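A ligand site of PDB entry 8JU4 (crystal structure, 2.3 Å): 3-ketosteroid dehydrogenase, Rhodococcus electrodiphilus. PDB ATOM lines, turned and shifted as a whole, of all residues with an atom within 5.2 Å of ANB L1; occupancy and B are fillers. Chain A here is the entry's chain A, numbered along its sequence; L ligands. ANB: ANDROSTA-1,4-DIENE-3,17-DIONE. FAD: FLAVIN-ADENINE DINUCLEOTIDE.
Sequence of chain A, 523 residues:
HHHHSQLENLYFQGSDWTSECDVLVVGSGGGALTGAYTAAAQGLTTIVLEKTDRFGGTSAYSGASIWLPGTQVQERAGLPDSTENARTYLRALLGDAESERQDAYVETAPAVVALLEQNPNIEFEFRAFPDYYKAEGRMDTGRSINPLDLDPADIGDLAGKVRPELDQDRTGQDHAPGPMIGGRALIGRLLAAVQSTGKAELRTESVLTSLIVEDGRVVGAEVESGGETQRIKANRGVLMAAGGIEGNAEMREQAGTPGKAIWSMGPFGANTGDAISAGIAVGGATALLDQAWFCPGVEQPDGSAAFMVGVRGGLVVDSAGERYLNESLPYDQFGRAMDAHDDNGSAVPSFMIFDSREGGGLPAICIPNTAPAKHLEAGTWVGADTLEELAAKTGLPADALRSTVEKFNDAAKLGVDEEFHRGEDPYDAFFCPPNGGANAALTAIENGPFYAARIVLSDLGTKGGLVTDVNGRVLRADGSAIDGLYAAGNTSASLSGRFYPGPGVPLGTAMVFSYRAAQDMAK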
ATOM      1  N   GLY A  63      22.714   5.051  18.787  1.00  0.00           N
ATOM      2  CA  GLY A  63      22.830   4.820  20.244  1.00  0.00           C
ATOM      3  C   GLY A  63      23.519   3.504  20.534  1.00  0.00           C
ATOM      4  O   GLY A  63      23.659   3.137  21.718  1.00  0.00           O
ATOM      5  N   SER A  65      22.622   0.586  20.300  1.00  0.00           N
ATOM      6  CA  SER A  65      21.798  -0.499  20.861  1.00  0.00           C
ATOM      7  C   SER A  65      21.862  -1.635  19.827  1.00  0.00           C
ATOM      8  O   SER A  65      21.762  -1.381  18.623  1.00  0.00           O
ATOM      9  CB  SER A  65      20.407   0.019  21.231  1.00  0.00           C
ATOM     10  OG  SER A  65      19.500  -1.044  21.387  1.00  0.00           O
ATOM     11  N   PHE A 129      15.576  -1.200  26.782  1.00  0.00           N
ATOM     12  CA  PHE A 129      14.877  -0.435  25.730  1.00  0.00           C
ATOM     13  C   PHE A 129      13.854  -1.417  25.167  1.00  0.00           C
ATOM     14  O   PHE A 129      14.237  -2.503  24.735  1.00  0.00           O
ATOM     15  CB  PHE A 129      15.903   0.109  24.712  1.00  0.00           C
ATOM     16  CG  PHE A 129      15.449   1.384  24.055  1.00  0.00           C
ATOM     17  CD1 PHE A 129      14.551   1.366  22.993  1.00  0.00           C
ATOM     18  CD2 PHE A 129      15.903   2.624  24.504  1.00  0.00           C
ATOM     19  CE1 PHE A 129      14.113   2.545  22.396  1.00  0.00           C
ATOM     20  CE2 PHE A 129      15.447   3.801  23.921  1.00  0.00           C
ATOM     21  CZ  PHE A 129      14.565   3.758  22.863  1.00  0.00           C
ATOM     22  N   TYR A 132       9.408  -3.675  20.133  1.00  0.00           N
ATOM     23  CA  TYR A 132       8.503  -2.663  19.515  1.00  0.00           C
ATOM     24  C   TYR A 132       7.112  -3.236  19.143  1.00  0.00           C
ATOM     25  O   TYR A 132       6.239  -2.409  18.825  1.00  0.00           O
ATOM     26  CB  TYR A 132       9.165  -2.065  18.273  1.00  0.00           C
ATOM     27  CG  TYR A 132      10.456  -1.318  18.487  1.00  0.00           C
ATOM     28  CD1 TYR A 132      10.801  -0.802  19.725  1.00  0.00           C
ATOM     29  CD2 TYR A 132      11.309  -1.058  17.415  1.00  0.00           C
ATOM     30  CE1 TYR A 132      11.969  -0.083  19.912  1.00  0.00           C
ATOM     31  CE2 TYR A 132      12.491  -0.345  17.584  1.00  0.00           C
ATOM     32  CZ  TYR A 132      12.829   0.160  18.840  1.00  0.00           C
ATOM     33  OH  TYR A 132      13.964   0.889  19.051  1.00  0.00           O
ATOM     34  N   PHE A 307      15.567  13.210  13.816  1.00  0.00           N
ATOM     35  CA  PHE A 307      14.926  11.982  14.359  1.00  0.00           C
ATOM     36  C   PHE A 307      14.125  12.362  15.608  1.00  0.00           C
ATOM     37  O   PHE A 307      14.759  12.912  16.523  1.00  0.00           O
ATOM     38  CB  PHE A 307      16.019  10.976  14.665  1.00  0.00           C
ATOM     39  CG  PHE A 307      15.569   9.661  15.236  1.00  0.00           C
ATOM     40  CD1 PHE A 307      14.267   9.201  15.029  1.00  0.00           C
ATOM     41  CD2 PHE A 307      16.453   8.860  15.928  1.00  0.00           C
ATOM     42  CE1 PHE A 307      13.883   7.950  15.479  1.00  0.00           C
ATOM     43  CE2 PHE A 307      16.045   7.617  16.399  1.00  0.00           C
ATOM     44  CZ  PHE A 307      14.751   7.161  16.182  1.00  0.00           C
ATOM     45  N   VAL A 309      12.138  10.889  18.624  1.00  0.00           N
ATOM     46  CA  VAL A 309      12.060   9.572  19.331  1.00  0.00           C
ATOM     47  C   VAL A 309      11.661   9.845  20.796  1.00  0.00           C
ATOM     48  O   VAL A 309      11.851  10.990  21.268  1.00  0.00           O
ATOM     49  CB  VAL A 309      13.389   8.791  19.192  1.00  0.00           C
ATOM     50  CG1 VAL A 309      14.545   9.481  19.904  1.00  0.00           C
ATOM     51  CG2 VAL A 309      13.265   7.355  19.699  1.00  0.00           C
ATOM     52  N   TYR A 331       8.949   4.422  16.363  1.00  0.00           N
ATOM     53  CA  TYR A 331       9.227   5.358  15.240  1.00  0.00           C
ATOM     54  C   TYR A 331       9.003   4.751  13.836  1.00  0.00           C
ATOM     55  O   TYR A 331       8.523   5.476  12.942  1.00  0.00           O
ATOM     56  CB  TYR A 331      10.644   5.923  15.382  1.00  0.00           C
ATOM     57  CG  TYR A 331      11.687   4.913  15.741  1.00  0.00           C
ATOM     58  CD1 TYR A 331      11.952   4.582  17.061  1.00  0.00           C
ATOM     59  CD2 TYR A 331      12.432   4.296  14.755  1.00  0.00           C
ATOM     60  CE1 TYR A 331      12.932   3.654  17.390  1.00  0.00           C
ATOM     61  CE2 TYR A 331      13.400   3.353  15.058  1.00  0.00           C
ATOM     62  CZ  TYR A 331      13.659   3.038  16.380  1.00  0.00           C
ATOM     63  OH  TYR A 331      14.589   2.082  16.637  1.00  0.00           O
ATOM     64  N   ILE A 365      12.643  13.556  22.353  1.00  0.00           N
ATOM     65  CA  ILE A 365      14.076  13.673  21.949  1.00  0.00           C
ATOM     66  C   ILE A 365      14.130  13.962  20.435  1.00  0.00           C
ATOM     67  O   ILE A 365      13.557  13.194  19.620  1.00  0.00           O
ATOM     68  CB  ILE A 365      14.865  12.409  22.352  1.00  0.00           C
ATOM     69  CG1 ILE A 365      14.642  12.109  23.846  1.00  0.00           C
ATOM     70  CG2 ILE A 365      16.332  12.536  22.019  1.00  0.00           C
ATOM     71  CD1 ILE A 365      14.851  10.658  24.221  1.00  0.00           C
ATOM     72  N   ILE A 367      16.985  14.618  17.419  1.00  0.00           N
ATOM     73  CA  ILE A 367      18.431  14.424  17.106  1.00  0.00           C
ATOM     74  C   ILE A 367      18.653  14.808  15.645  1.00  0.00           C
ATOM     75  O   ILE A 367      18.228  14.092  14.742  1.00  0.00           O
ATOM     76  CB  ILE A 367      18.845  12.989  17.438  1.00  0.00           C
ATOM     77  CG1 ILE A 367      18.352  12.581  18.838  1.00  0.00           C
ATOM     78  CG2 ILE A 367      20.355  12.768  17.293  1.00  0.00           C
ATOM     79  CD1 ILE A 367      18.609  11.107  19.177  1.00  0.00           C
ATOM     80  N   LEU A 460      16.329   6.303   9.043  1.00  0.00           N
ATOM     81  CA  LEU A 460      17.624   5.988   9.661  1.00  0.00           C
ATOM     82  C   LEU A 460      18.429   5.121   8.696  1.00  0.00           C
ATOM     83  O   LEU A 460      19.136   4.199   9.184  1.00  0.00           O
ATOM     84  CB  LEU A 460      17.364   5.219  10.960  1.00  0.00           C
ATOM     85  CG  LEU A 460      16.452   5.880  11.958  1.00  0.00           C
ATOM     86  CD1 LEU A 460      16.366   5.021  13.194  1.00  0.00           C
ATOM     87  CD2 LEU A 460      16.939   7.269  12.320  1.00  0.00           C
ATOM     88  N   TYR A 500      10.413  -3.412  11.812  1.00  0.00           N
ATOM     89  CA  TYR A 500      11.495  -2.994  12.722  1.00  0.00           C
ATOM     90  C   TYR A 500      11.204  -3.649  14.068  1.00  0.00           C
ATOM     91  O   TYR A 500      10.518  -3.093  14.905  1.00  0.00           O
ATOM     92  CB  TYR A 500      11.578  -1.460  12.718  1.00  0.00           C
ATOM     93  CG  TYR A 500      12.896  -0.850  13.141  1.00  0.00           C
ATOM     94  CD1 TYR A 500      13.687  -1.400  14.141  1.00  0.00           C
ATOM     95  CD2 TYR A 500      13.320   0.342  12.586  1.00  0.00           C
ATOM     96  CE1 TYR A 500      14.868  -0.783  14.569  1.00  0.00           C
ATOM     97  CE2 TYR A 500      14.511   0.959  12.973  1.00  0.00           C
ATOM     98  CZ  TYR A 500      15.275   0.409  13.989  1.00  0.00           C
ATOM     99  OH  TYR A 500      16.418   1.050  14.375  1.00  0.00           O
ATOM    100  N   GLY A 502      12.702  -4.534  16.948  1.00  0.00           N
ATOM    101  CA  GLY A 502      13.146  -3.988  18.242  1.00  0.00           C
ATOM    102  C   GLY A 502      14.420  -3.172  18.123  1.00  0.00           C
ATOM    103  O   GLY A 502      15.028  -3.123  17.053  1.00  0.00           O
ATOM    104  N   PRO A 503      14.894  -2.548  19.232  1.00  0.00           N
ATOM    105  CA  PRO A 503      16.056  -1.673  19.158  1.00  0.00           C
ATOM    106  C   PRO A 503      17.267  -2.529  18.756  1.00  0.00           C
ATOM    107  O   PRO A 503      17.441  -3.600  19.308  1.00  0.00           O
ATOM    108  CB  PRO A 503      16.178  -1.121  20.589  1.00  0.00           C
ATOM    109  CG  PRO A 503      15.618  -2.266  21.443  1.00  0.00           C
ATOM    110  CD  PRO A 503      14.449  -2.756  20.625  1.00  0.00           C
ATOM    111  N   GLY A 504      18.050  -2.073  17.789  1.00  0.00           N
ATOM    112  CA  GLY A 504      19.357  -2.685  17.504  1.00  0.00           C
ATOM    113  C   GLY A 504      19.284  -3.729  16.402  1.00  0.00           C
ATOM    114  O   GLY A 504      20.290  -4.398  16.200  1.00  0.00           O
ATOM    115  N   VAL A 505      18.162  -3.870  15.701  1.00  0.00           N
ATOM    116  CA  VAL A 505      18.053  -4.867  14.615  1.00  0.00           C
ATOM    117  C   VAL A 505      18.917  -4.459  13.419  1.00  0.00           C
ATOM    118  O   VAL A 505      19.530  -5.305  12.802  1.00  0.00           O
ATOM    119  CB  VAL A 505      16.598  -5.126  14.197  1.00  0.00           C
ATOM    120  CG1 VAL A 505      16.524  -5.904  12.899  1.00  0.00           C
ATOM    121  CG2 VAL A 505      15.853  -5.880  15.290  1.00  0.00           C
ATOM    122  N   PRO A 506      18.955  -3.185  12.979  1.00  0.00           N
ATOM    123  CA  PRO A 506      19.850  -2.783  11.892  1.00  0.00           C
ATOM    124  C   PRO A 506      21.313  -3.150  12.217  1.00  0.00           C
ATOM    125  O   PRO A 506      21.907  -3.852  11.448  1.00  0.00           O
ATOM    126  CB  PRO A 506      19.605  -1.272  11.740  1.00  0.00           C
ATOM    127  CG  PRO A 506      18.195  -1.105  12.236  1.00  0.00           C
ATOM    128  CD  PRO A 506      18.109  -2.066  13.412  1.00  0.00           C
HETATM  129  C1  ANB L   1      17.408   4.073  17.773  1.00  0.00           C
HETATM  130  C10 ANB L   1      17.261   3.961  19.259  1.00  0.00           C
HETATM  131  C11 ANB L   1      18.121   6.395  19.523  1.00  0.00           C
HETATM  132  C12 ANB L   1      19.035   7.372  20.262  1.00  0.00           C
HETATM  133  C13 ANB L   1      18.899   7.201  21.764  1.00  0.00           C
HETATM  134  C14 ANB L   1      19.260   5.761  22.135  1.00  0.00           C
HETATM  135  C15 ANB L   1      19.488   5.784  23.651  1.00  0.00           C
HETATM  136  C16 ANB L   1      20.112   7.172  23.896  1.00  0.00           C
HETATM  137  C17 ANB L   1      19.910   7.962  22.614  1.00  0.00           C
HETATM  138  C18 ANB L   1      17.522   7.628  22.292  1.00  0.00           C
HETATM  139  C19 ANB L   1      15.775   4.264  19.562  1.00  0.00           C
HETATM  140  C2  ANB L   1      17.449   3.029  16.948  1.00  0.00           C
HETATM  141  C3  ANB L   1      17.599   1.678  17.438  1.00  0.00           C
HETATM  142  C4  ANB L   1      17.753   1.539  18.877  1.00  0.00           C
HETATM  143  C5  ANB L   1      17.585   2.556  19.729  1.00  0.00           C
HETATM  144  C6  ANB L   1      17.715   2.349  21.217  1.00  0.00           C
HETATM  145  C7  ANB L   1      18.684   3.330  21.849  1.00  0.00           C
HETATM  146  C8  ANB L   1      18.297   4.764  21.502  1.00  0.00           C
HETATM  147  C9  ANB L   1      18.271   4.935  19.962  1.00  0.00           C
HETATM  148  O1  ANB L   1      17.587   0.696  16.670  1.00  0.00           O
HETATM  149  O2  ANB L   1      20.471   8.996  22.294  1.00  0.00           O
HETATM  150  PA  FAD L   2      26.705   3.054   7.823  1.00  0.00           P
HETATM  151  O1A FAD L   2      26.821   2.781   9.283  1.00  0.00           O
HETATM  152  O2A FAD L   2      26.202   4.415   7.398  1.00  0.00           O
HETATM  153  O5B FAD L   2      28.104   2.732   7.133  1.00  0.00           O
HETATM  154  C5B FAD L   2      28.302   3.011   5.716  1.00  0.00           C
HETATM  155  C4B FAD L   2      29.677   3.594   5.484  1.00  0.00           C
HETATM  156  O4B FAD L   2      30.093   3.279   4.113  1.00  0.00           O
HETATM  157  C3B FAD L   2      29.742   5.113   5.613  1.00  0.00           C
HETATM  158  O3B FAD L   2      30.824   5.582   6.408  1.00  0.00           O
HETATM  159  C2B FAD L   2      29.894   5.587   4.167  1.00  0.00           C
HETATM  160  O2B FAD L   2      30.582   6.815   4.076  1.00  0.00           O
HETATM  161  C1B FAD L   2      30.680   4.430   3.562  1.00  0.00           C
HETATM  162  N9A FAD L   2      30.615   4.381   2.115  1.00  0.00           N
HETATM  163  C8A FAD L   2      29.520   4.673   1.317  1.00  0.00           C
HETATM  164  N7A FAD L   2      29.774   4.536   0.044  1.00  0.00           N
HETATM  165  C5A FAD L   2      31.101   4.105   0.000  1.00  0.00           C
HETATM  166  C6A FAD L   2      31.939   3.805  -1.081  1.00  0.00           C
HETATM  167  N6A FAD L   2      31.551   3.921  -2.348  1.00  0.00           N
HETATM  168  N1A FAD L   2      33.194   3.406  -0.778  1.00  0.00           N
HETATM  169  C2A FAD L   2      33.568   3.332   0.513  1.00  0.00           C
HETATM  170  N3A FAD L   2      32.879   3.623   1.600  1.00  0.00           N
HETATM  171  C4A FAD L   2      31.632   4.002   1.266  1.00  0.00           C
HETATM  172  N1  FAD L   2      20.369   1.120  14.694  1.00  0.00           N
HETATM  173  C2  FAD L   2      20.611   0.197  15.639  1.00  0.00           C
HETATM  174  O2  FAD L   2      20.654  -1.009  15.358  1.00  0.00           O
HETATM  175  N3  FAD L   2      20.779   0.526  16.945  1.00  0.00           N
HETATM  176  C4  FAD L   2      20.612   1.796  17.408  1.00  0.00           C
HETATM  177  O4  FAD L   2      20.817   2.015  18.606  1.00  0.00           O
HETATM  178  C4X FAD L   2      20.418   2.821  16.427  1.00  0.00           C
HETATM  179  N5  FAD L   2      20.304   4.068  16.801  1.00  0.00           N
HETATM  180  C5X FAD L   2      20.235   5.031  15.822  1.00  0.00           C
HETATM  181  C6  FAD L   2      20.236   6.373  16.213  1.00  0.00           C
HETATM  182  C7  FAD L   2      20.307   7.394  15.297  1.00  0.00           C
HETATM  183  C7M FAD L   2      20.318   8.828  15.790  1.00  0.00           C
HETATM  184  C8  FAD L   2      20.336   7.080  13.921  1.00  0.00           C
HETATM  185  C8M FAD L   2      20.333   8.166  12.883  1.00  0.00           C
HETATM  186  C9  FAD L   2      20.197   5.758  13.520  1.00  0.00           C
HETATM  187  C9A FAD L   2      20.210   4.714  14.448  1.00  0.00           C
HETATM  188  N10 FAD L   2      20.173   3.368  14.083  1.00  0.00           N
HETATM  189  C10 FAD L   2      20.308   2.383  15.051  1.00  0.00           C
HETATM  190  C1' FAD L   2      20.167   2.974  12.657  1.00  0.00           C
HETATM  191  C2' FAD L   2      21.523   2.573  12.178  1.00  0.00           C
HETATM  192  O2' FAD L   2      22.476   3.605  12.568  1.00  0.00           O
HETATM  193  C3' FAD L   2      21.677   2.366  10.659  1.00  0.00           C
HETATM  194  O3' FAD L   2      20.549   1.892   9.968  1.00  0.00           O
HETATM  195  C4' FAD L   2      22.797   1.375  10.466  1.00  0.00           C
HETATM  196  O4' FAD L   2      23.903   1.790  11.279  1.00  0.00           O
HETATM  197  C5' FAD L   2      23.235   1.303   9.034  1.00  0.00           C
HETATM  198  O5' FAD L   2      24.576   0.789   8.999  1.00  0.00           O
HETATM  199  P   FAD L   2      25.251   0.506   7.567  1.00  0.00           P
HETATM  200  O1P FAD L   2      26.407  -0.342   7.843  1.00  0.00           O
HETATM  201  O2P FAD L   2      24.179   0.044   6.620  1.00  0.00           O
HETATM  202  O3P FAD L   2      25.735   1.975   7.160  1.00  0.00           O
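The backbone NH of Gly 504 sits at hydrogen-bond distance from an oxygen (O1) of ANB L1. O of Ser 65 sits at hydrogen-bond distance from N3 of FAD L2, 2.7 Å away. The backbone carbonyl oxygen of Leu 460 is in hydrogen-bond range of an oxygen (O3') of FAD L2, 2.8 Å away. N5 of FAD L2 is in hydrogen-bond range of N of Gly 63. The side-chain hydroxyl (OH) of Tyr 500 lies within hydrogen-bond range of an oxygen (O1) of ANB L1, at 2.6 Å. An oxygen (O4) of FAD L2 lies within hydrogen-bond range of the backbone NH (N) of Ser 65, 2.9 Å away. OH of Tyr 331 sits close to O1 of ANB L1, 3.3 Å away.
An oxygen (O1) of ANB L1 sits at hydrogen-bond distance from a nitrogen (N3) of FAD L2 (3.2 Å).
The side-chain hydroxyl (OH) of Tyr 331 lies within hydrogen-bond range of the side-chain hydroxyl (OH) of Tyr 500. O of Phe 307 is in hydrogen-bond range of N of Ile 367, 2.9 Å away. OH of Tyr 331 is in hydrogen-bond range of OH of Tyr 132 (2.8 Å). The backbone carbonyl oxygen (O) of Ile 365 is in hydrogen-bond range of the backbone NH (N) of Val 309 (2.9 Å).
Ser 65 touches ANB L1 (CB to C6, 3.6 Å). Phe 129 touches ANB L1 (CZ to C19, 3.6 Å). Tyr 132 touches ANB L1 (OH to C4, 3.8 Å). CE2 of Phe 307 touches C11 of ANB L1, 3.9 Å away. Val 309 touches ANB L1 (CG2 to C19, 3.98 Å). Ile 367 touches ANB L1. CB of Pro 503 touches C4 of ANB L1 (3.5 Å). Hydrophobic or aromatic side chains that line ANB L1: Phe 129, Phe 307, Val 309, Tyr 331, Ile 367, Tyr 500 and Pro 503. Of the 16 residues printed, 10 come within 4 Å of ANB L1. The nearest printed residue that does not touch ANB L1 is Gly 63 (4.1 Å).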
